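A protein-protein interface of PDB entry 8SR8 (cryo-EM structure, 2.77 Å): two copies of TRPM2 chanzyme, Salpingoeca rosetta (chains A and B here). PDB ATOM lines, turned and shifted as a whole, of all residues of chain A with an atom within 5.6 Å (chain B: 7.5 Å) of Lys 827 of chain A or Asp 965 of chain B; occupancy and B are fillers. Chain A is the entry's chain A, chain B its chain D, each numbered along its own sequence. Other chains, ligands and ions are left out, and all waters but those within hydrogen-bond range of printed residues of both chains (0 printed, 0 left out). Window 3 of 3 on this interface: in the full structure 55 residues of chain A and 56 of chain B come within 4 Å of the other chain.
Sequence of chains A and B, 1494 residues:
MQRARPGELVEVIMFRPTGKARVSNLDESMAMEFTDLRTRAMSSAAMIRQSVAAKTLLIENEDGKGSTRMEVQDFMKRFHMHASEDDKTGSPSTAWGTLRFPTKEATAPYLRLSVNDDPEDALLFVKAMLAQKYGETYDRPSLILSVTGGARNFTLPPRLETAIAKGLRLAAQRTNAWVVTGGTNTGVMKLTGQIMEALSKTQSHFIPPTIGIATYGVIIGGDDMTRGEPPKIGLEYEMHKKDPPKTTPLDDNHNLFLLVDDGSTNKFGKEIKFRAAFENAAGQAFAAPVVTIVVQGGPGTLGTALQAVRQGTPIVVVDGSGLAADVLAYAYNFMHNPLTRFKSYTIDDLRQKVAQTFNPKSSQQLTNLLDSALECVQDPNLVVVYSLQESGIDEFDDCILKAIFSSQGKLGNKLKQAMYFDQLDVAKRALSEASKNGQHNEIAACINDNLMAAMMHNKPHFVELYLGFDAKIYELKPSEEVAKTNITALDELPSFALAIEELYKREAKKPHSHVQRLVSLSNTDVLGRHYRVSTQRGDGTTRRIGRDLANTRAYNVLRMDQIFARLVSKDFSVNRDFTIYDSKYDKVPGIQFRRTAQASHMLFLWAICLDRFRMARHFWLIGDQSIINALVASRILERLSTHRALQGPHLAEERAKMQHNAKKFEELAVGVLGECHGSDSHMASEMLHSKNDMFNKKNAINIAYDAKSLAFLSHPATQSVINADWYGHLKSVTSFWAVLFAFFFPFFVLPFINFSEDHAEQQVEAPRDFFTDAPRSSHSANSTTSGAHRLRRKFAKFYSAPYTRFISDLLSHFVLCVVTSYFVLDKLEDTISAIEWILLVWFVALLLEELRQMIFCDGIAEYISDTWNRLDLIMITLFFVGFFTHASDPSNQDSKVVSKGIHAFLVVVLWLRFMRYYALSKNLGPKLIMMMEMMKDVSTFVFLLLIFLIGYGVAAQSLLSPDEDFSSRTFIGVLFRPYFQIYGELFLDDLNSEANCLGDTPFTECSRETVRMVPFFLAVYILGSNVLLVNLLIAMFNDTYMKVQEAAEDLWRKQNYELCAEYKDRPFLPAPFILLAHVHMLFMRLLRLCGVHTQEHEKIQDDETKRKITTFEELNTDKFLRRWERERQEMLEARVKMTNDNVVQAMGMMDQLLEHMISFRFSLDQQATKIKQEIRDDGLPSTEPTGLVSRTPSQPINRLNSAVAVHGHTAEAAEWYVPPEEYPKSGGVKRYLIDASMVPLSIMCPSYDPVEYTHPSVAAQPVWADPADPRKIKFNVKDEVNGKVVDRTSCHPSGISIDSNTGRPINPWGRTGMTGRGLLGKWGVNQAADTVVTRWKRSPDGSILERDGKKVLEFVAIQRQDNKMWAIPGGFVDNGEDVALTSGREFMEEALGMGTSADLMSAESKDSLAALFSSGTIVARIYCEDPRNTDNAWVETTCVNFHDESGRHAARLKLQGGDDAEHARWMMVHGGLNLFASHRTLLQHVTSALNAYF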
ATOM      1  N   PHE A 823      21.713  17.939  12.761  1.00  0.00           N
ATOM      2  CA  PHE A 823      22.821  18.423  11.932  1.00  0.00           C
ATOM      3  C   PHE A 823      23.670  17.280  11.380  1.00  0.00           C
ATOM      4  O   PHE A 823      24.091  17.318  10.218  1.00  0.00           O
ATOM      5  CB  PHE A 823      23.679  19.379  12.757  1.00  0.00           C
ATOM      6  CG  PHE A 823      24.983  19.735  12.122  1.00  0.00           C
ATOM      7  CD1 PHE A 823      25.001  20.541  10.980  1.00  0.00           C
ATOM      8  CD2 PHE A 823      26.197  19.299  12.690  1.00  0.00           C
ATOM      9  CE1 PHE A 823      26.208  20.897  10.384  1.00  0.00           C
ATOM     10  CE2 PHE A 823      27.415  19.638  12.100  1.00  0.00           C
ATOM     11  CZ  PHE A 823      27.415  20.435  10.945  1.00  0.00           C
ATOM     12  N   LEU A 825      22.652  14.020  11.144  1.00  0.00           N
ATOM     13  CA  LEU A 825      21.830  13.152  10.280  1.00  0.00           C
ATOM     14  C   LEU A 825      21.530  13.746   8.900  1.00  0.00           C
ATOM     15  O   LEU A 825      21.560  13.020   7.902  1.00  0.00           O
ATOM     16  CB  LEU A 825      20.523  12.784  10.966  1.00  0.00           C
ATOM     17  CG  LEU A 825      20.655  11.730  12.050  1.00  0.00           C
ATOM     18  CD1 LEU A 825      19.363  11.614  12.797  1.00  0.00           C
ATOM     19  CD2 LEU A 825      21.075  10.427  11.486  1.00  0.00           C
ATOM     20  N   ASP A 826      21.175  15.029   8.831  1.00  0.00           N
ATOM     21  CA  ASP A 826      20.911  15.702   7.561  1.00  0.00           C
ATOM     22  C   ASP A 826      22.228  15.947   6.829  1.00  0.00           C
ATOM     23  O   ASP A 826      23.284  16.032   7.461  1.00  0.00           O
ATOM     24  CB  ASP A 826      20.163  17.017   7.798  1.00  0.00           C
ATOM     25  CG  ASP A 826      19.580  17.617   6.541  1.00  0.00           C
ATOM     26  OD1 ASP A 826      18.765  16.942   5.884  1.00  0.00           O
ATOM     27  OD2 ASP A 826      19.936  18.764   6.210  1.00  0.00           O
ATOM     28  N   LYS A 827      22.171  15.942   5.491  1.00  0.00           N
ATOM     29  CA  LYS A 827      23.353  16.111   4.653  1.00  0.00           C
ATOM     30  C   LYS A 827      23.917  17.529   4.750  1.00  0.00           C
ATOM     31  O   LYS A 827      23.206  18.501   5.022  1.00  0.00           O
ATOM     32  CB  LYS A 827      23.053  15.746   3.195  1.00  0.00           C
ATOM     33  CG  LYS A 827      22.148  16.685   2.413  1.00  0.00           C
ATOM     34  CD  LYS A 827      21.957  16.215   0.992  1.00  0.00           C
ATOM     35  CE  LYS A 827      23.226  16.403   0.190  1.00  0.00           C
ATOM     36  NZ  LYS A 827      23.041  15.990  -1.224  1.00  0.00           N
ATOM     37  N   LEU A 828      25.231  17.613   4.632  1.00  0.00           N
ATOM     38  CA  LEU A 828      25.919  18.888   4.646  1.00  0.00           C
ATOM     39  C   LEU A 828      25.774  19.576   3.300  1.00  0.00           C
ATOM     40  O   LEU A 828      25.710  18.928   2.256  1.00  0.00           O
ATOM     41  CB  LEU A 828      27.387  18.683   4.994  1.00  0.00           C
ATOM     42  CG  LEU A 828      27.737  18.362   6.434  1.00  0.00           C
ATOM     43  CD1 LEU A 828      29.140  17.836   6.498  1.00  0.00           C
ATOM     44  CD2 LEU A 828      27.635  19.614   7.227  1.00  0.00           C
ATOM     45  N   GLU A 829      25.685  20.893   3.333  1.00  0.00           N
ATOM     46  CA  GLU A 829      25.583  21.679   2.118  1.00  0.00           C
ATOM     47  C   GLU A 829      26.974  22.017   1.606  1.00  0.00           C
ATOM     48  O   GLU A 829      27.984  21.776   2.266  1.00  0.00           O
ATOM     49  CB  GLU A 829      24.781  22.953   2.356  1.00  0.00           C
ATOM     50  CG  GLU A 829      23.412  22.731   2.952  1.00  0.00           C
ATOM     51  CD  GLU A 829      22.765  24.024   3.406  1.00  0.00           C
ATOM     52  OE1 GLU A 829      23.459  25.061   3.437  1.00  0.00           O
ATOM     53  OE2 GLU A 829      21.559  24.005   3.728  1.00  0.00           O
ATOM     54  N   LYS A 896      33.296  16.172   3.667  1.00  0.00           N
ATOM     55  CA  LYS A 896      31.945  15.985   4.209  1.00  0.00           C
ATOM     56  C   LYS A 896      31.800  14.635   4.908  1.00  0.00           C
ATOM     57  O   LYS A 896      31.242  14.561   6.018  1.00  0.00           O
ATOM     58  CB  LYS A 896      30.977  16.065   3.027  1.00  0.00           C
ATOM     59  CG  LYS A 896      30.701  17.419   2.411  1.00  0.00           C
ATOM     60  CD  LYS A 896      29.525  17.355   1.425  1.00  0.00           C
ATOM     61  CE  LYS A 896      28.258  16.731   1.923  1.00  0.00           C
ATOM     62  NZ  LYS A 896      27.346  16.373   0.800  1.00  0.00           N
ATOM     63  N   LYS A 900      31.496  14.119   9.042  1.00  0.00           N
ATOM     64  CA  LYS A 900      30.398  13.362   9.651  1.00  0.00           C
ATOM     65  C   LYS A 900      30.907  12.175  10.472  1.00  0.00           C
ATOM     66  O   LYS A 900      30.256  11.794  11.457  1.00  0.00           O
ATOM     67  CB  LYS A 900      29.402  12.897   8.598  1.00  0.00           C
ATOM     68  CG  LYS A 900      28.410  13.961   8.225  1.00  0.00           C
ATOM     69  CD  LYS A 900      27.315  13.401   7.364  1.00  0.00           C
ATOM     70  CE  LYS A 900      26.314  14.469   7.022  1.00  0.00           C
ATOM     71  NZ  LYS A 900      25.849  15.154   8.247  1.00  0.00           N
ATOM     72  N   SER B 961      24.474   6.437   6.051  1.00  0.00           N
ATOM     73  CA  SER B 961      23.952   7.288   4.978  1.00  0.00           C
ATOM     74  C   SER B 961      24.357   8.742   5.193  1.00  0.00           C
ATOM     75  O   SER B 961      23.570   9.538   5.721  1.00  0.00           O
ATOM     76  CB  SER B 961      22.432   7.181   4.901  1.00  0.00           C
ATOM     77  OG  SER B 961      22.030   5.831   4.806  1.00  0.00           O
ATOM     78  N   PRO B 962      25.577   9.130   4.799  1.00  0.00           N
ATOM     79  CA  PRO B 962      26.033  10.500   5.051  1.00  0.00           C
ATOM     80  C   PRO B 962      25.615  11.522   4.011  1.00  0.00           C
ATOM     81  O   PRO B 962      26.004  12.687   4.141  1.00  0.00           O
ATOM     82  CB  PRO B 962      27.563  10.355   5.024  1.00  0.00           C
ATOM     83  CG  PRO B 962      27.840   8.904   4.985  1.00  0.00           C
ATOM     84  CD  PRO B 962      26.688   8.340   4.251  1.00  0.00           C
ATOM     85  N   ASP B 963      24.863  11.156   2.982  1.00  0.00           N
ATOM     86  CA  ASP B 963      24.508  12.106   1.933  1.00  0.00           C
ATOM     87  C   ASP B 963      23.033  12.009   1.594  1.00  0.00           C
ATOM     88  O   ASP B 963      22.637  11.955   0.430  1.00  0.00           O
ATOM     89  CB  ASP B 963      25.360  11.883   0.691  1.00  0.00           C
ATOM     90  N   GLU B 964      22.196  11.989   2.619  1.00  0.00           N
ATOM     91  CA  GLU B 964      20.764  11.838   2.446  1.00  0.00           C
ATOM     92  C   GLU B 964      20.052  12.943   3.205  1.00  0.00           C
ATOM     93  O   GLU B 964      20.493  13.336   4.288  1.00  0.00           O
ATOM     94  CB  GLU B 964      20.282  10.474   2.939  1.00  0.00           C
ATOM     95  N   ASP B 965      19.002  13.489   2.588  1.00  0.00           N
ATOM     96  CA  ASP B 965      18.116  14.451   3.234  1.00  0.00           C
ATOM     97  C   ASP B 965      17.349  13.804   4.374  1.00  0.00           C
ATOM     98  O   ASP B 965      17.065  12.602   4.328  1.00  0.00           O
ATOM     99  CB  ASP B 965      17.126  15.028   2.228  1.00  0.00           C
ATOM    100  CG  ASP B 965      17.758  16.029   1.301  1.00  0.00           C
ATOM    101  OD1 ASP B 965      18.688  16.732   1.738  1.00  0.00           O
ATOM    102  OD2 ASP B 965      17.328  16.115   0.133  1.00  0.00           O
ATOM    103  N   PHE B 966      17.147  14.577   5.447  1.00  0.00           N
ATOM    104  CA  PHE B 966      16.393  14.129   6.612  1.00  0.00           C
ATOM    105  C   PHE B 966      14.929  13.945   6.219  1.00  0.00           C
ATOM    106  O   PHE B 966      14.338  14.777   5.529  1.00  0.00           O
ATOM    107  CB  PHE B 966      16.577  15.123   7.775  1.00  0.00           C
ATOM    108  CG  PHE B 966      16.068  14.642   9.138  1.00  0.00           C
ATOM    109  CD1 PHE B 966      14.723  14.793   9.559  1.00  0.00           C
ATOM    110  CD2 PHE B 966      16.976  14.007   9.997  1.00  0.00           C
ATOM    111  CE1 PHE B 966      14.305  14.318  10.808  1.00  0.00           C
ATOM    112  CE2 PHE B 966      16.571  13.531  11.252  1.00  0.00           C
ATOM    113  CZ  PHE B 966      15.236  13.690  11.649  1.00  0.00           C
ATOM    114  N   SER B 967      14.359  12.841   6.676  1.00  0.00           N
ATOM    115  CA  SER B 967      12.974  12.493   6.429  1.00  0.00           C
ATOM    116  C   SER B 967      12.516  11.648   7.602  1.00  0.00           C
ATOM    117  O   SER B 967      13.225  11.526   8.603  1.00  0.00           O
ATOM    118  CB  SER B 967      12.816  11.754   5.103  1.00  0.00           C
ATOM    119  OG  SER B 967      13.669  10.630   5.054  1.00  0.00           O
ATOM    120  N   SER B 968      11.275  11.158   7.511  1.00  0.00           N
ATOM    121  CA  SER B 968      10.718  10.250   8.515  1.00  0.00           C
ATOM    122  C   SER B 968      11.443   8.907   8.563  1.00  0.00           C
ATOM    123  O   SER B 968      11.584   8.335   9.651  1.00  0.00           O
ATOM    124  CB  SER B 968       9.235  10.030   8.246  1.00  0.00           C
ATOM    125  OG  SER B 968       9.046   9.446   6.974  1.00  0.00           O
ATOM    126  N   ARG B 969      11.953   8.444   7.403  1.00  0.00           N
ATOM    127  CA  ARG B 969      12.739   7.215   7.259  1.00  0.00           C
ATOM    128  C   ARG B 969      14.057   7.257   8.019  1.00  0.00           C
ATOM    129  O   ARG B 969      14.541   6.204   8.451  1.00  0.00           O
ATOM    130  CB  ARG B 969      13.031   6.958   5.787  1.00  0.00           C
ATOM    131  CG  ARG B 969      11.811   6.873   4.897  1.00  0.00           C
ATOM    132  CD  ARG B 969      12.121   6.610   3.406  1.00  0.00           C
ATOM    133  NE  ARG B 969      13.128   5.585   3.130  1.00  0.00           N
ATOM    134  CZ  ARG B 969      14.348   5.822   2.662  1.00  0.00           C
ATOM    135  NH1 ARG B 969      14.758   7.050   2.394  1.00  0.00           N
ATOM    136  NH2 ARG B 969      15.178   4.802   2.467  1.00  0.00           N
ATOM    137  N   THR B 970      14.658   8.452   8.126  1.00  0.00           N
ATOM    138  CA  THR B 970      15.863   8.686   8.920  1.00  0.00           C
ATOM    139  C   THR B 970      15.600   8.435  10.405  1.00  0.00           C
ATOM    140  O   THR B 970      16.405   7.777  11.073  1.00  0.00           O
ATOM    141  CB  THR B 970      16.352  10.114   8.675  1.00  0.00           C
ATOM    142  OG1 THR B 970      16.525  10.311   7.271  1.00  0.00           O
ATOM    143  CG2 THR B 970      17.683  10.369   9.329  1.00  0.00           C
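Of chain B, only Glu 964 and Asp 965 come within 4 Å of Lys 827 of chain A.
Asp 965 of chain B touches just these residues of chain A: Asp 826 (3.7 Å) and Lys 827 (3.4 Å).
Of the printed residues of chain A, Pro 962 of chain B touches Lys 900.
Of the printed residues of chain B, Leu 825 of chain A touches Glu 964 and Phe 966.
Thr 970 of chain B touches none of the printed residues of chain A.
The nearest residue of chain A that does not touch Asp 965 of chain B is Leu 825 of chain A (5.5 Å).
The nearest printed residue of chain A that does not touch Pro 962 of chain B is Lys 827 of chain A (4.4 Å).
NZ of Lys 900 of chain A sits at hydrogen-bond distance from O of Phe 823 of chain A.
O of Asp 826 of chain A is in hydrogen-bond range of NZ of Lys 900 of chain A, at 2.8 Å.
Among the printed residues, merely in contact across the chains: Leu 825 of chain A with Glu 964 of chain B (3.8 Å), Leu 825 of chain A with Phe 966 of chain B (3.7 Å), Asp 826 of chain A with Asp 965 of chain B (3.7 Å), Lys 827 of chain A with Asp 965 of chain B (3.4 Å) and Lys 900 of chain A with Pro 962 of chain B (3.4 Å).
The side-chain carboxylate (OD1) of Asp 826 of chain A is in hydrogen-bond range of the backbone NH (N) of Phe 966 of chain B.
N of Lys 827 of chain A sits at hydrogen-bond distance from O of Glu 964 of chain B (3.3 Å).
No position is printed for both chains.
Of the 7 pairs that touch across the chains among the printed residues, none has its exchanged pair printed and touching as well.
Of the 10 printed residues of chain B, 4 touch a printed residue of chain A.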
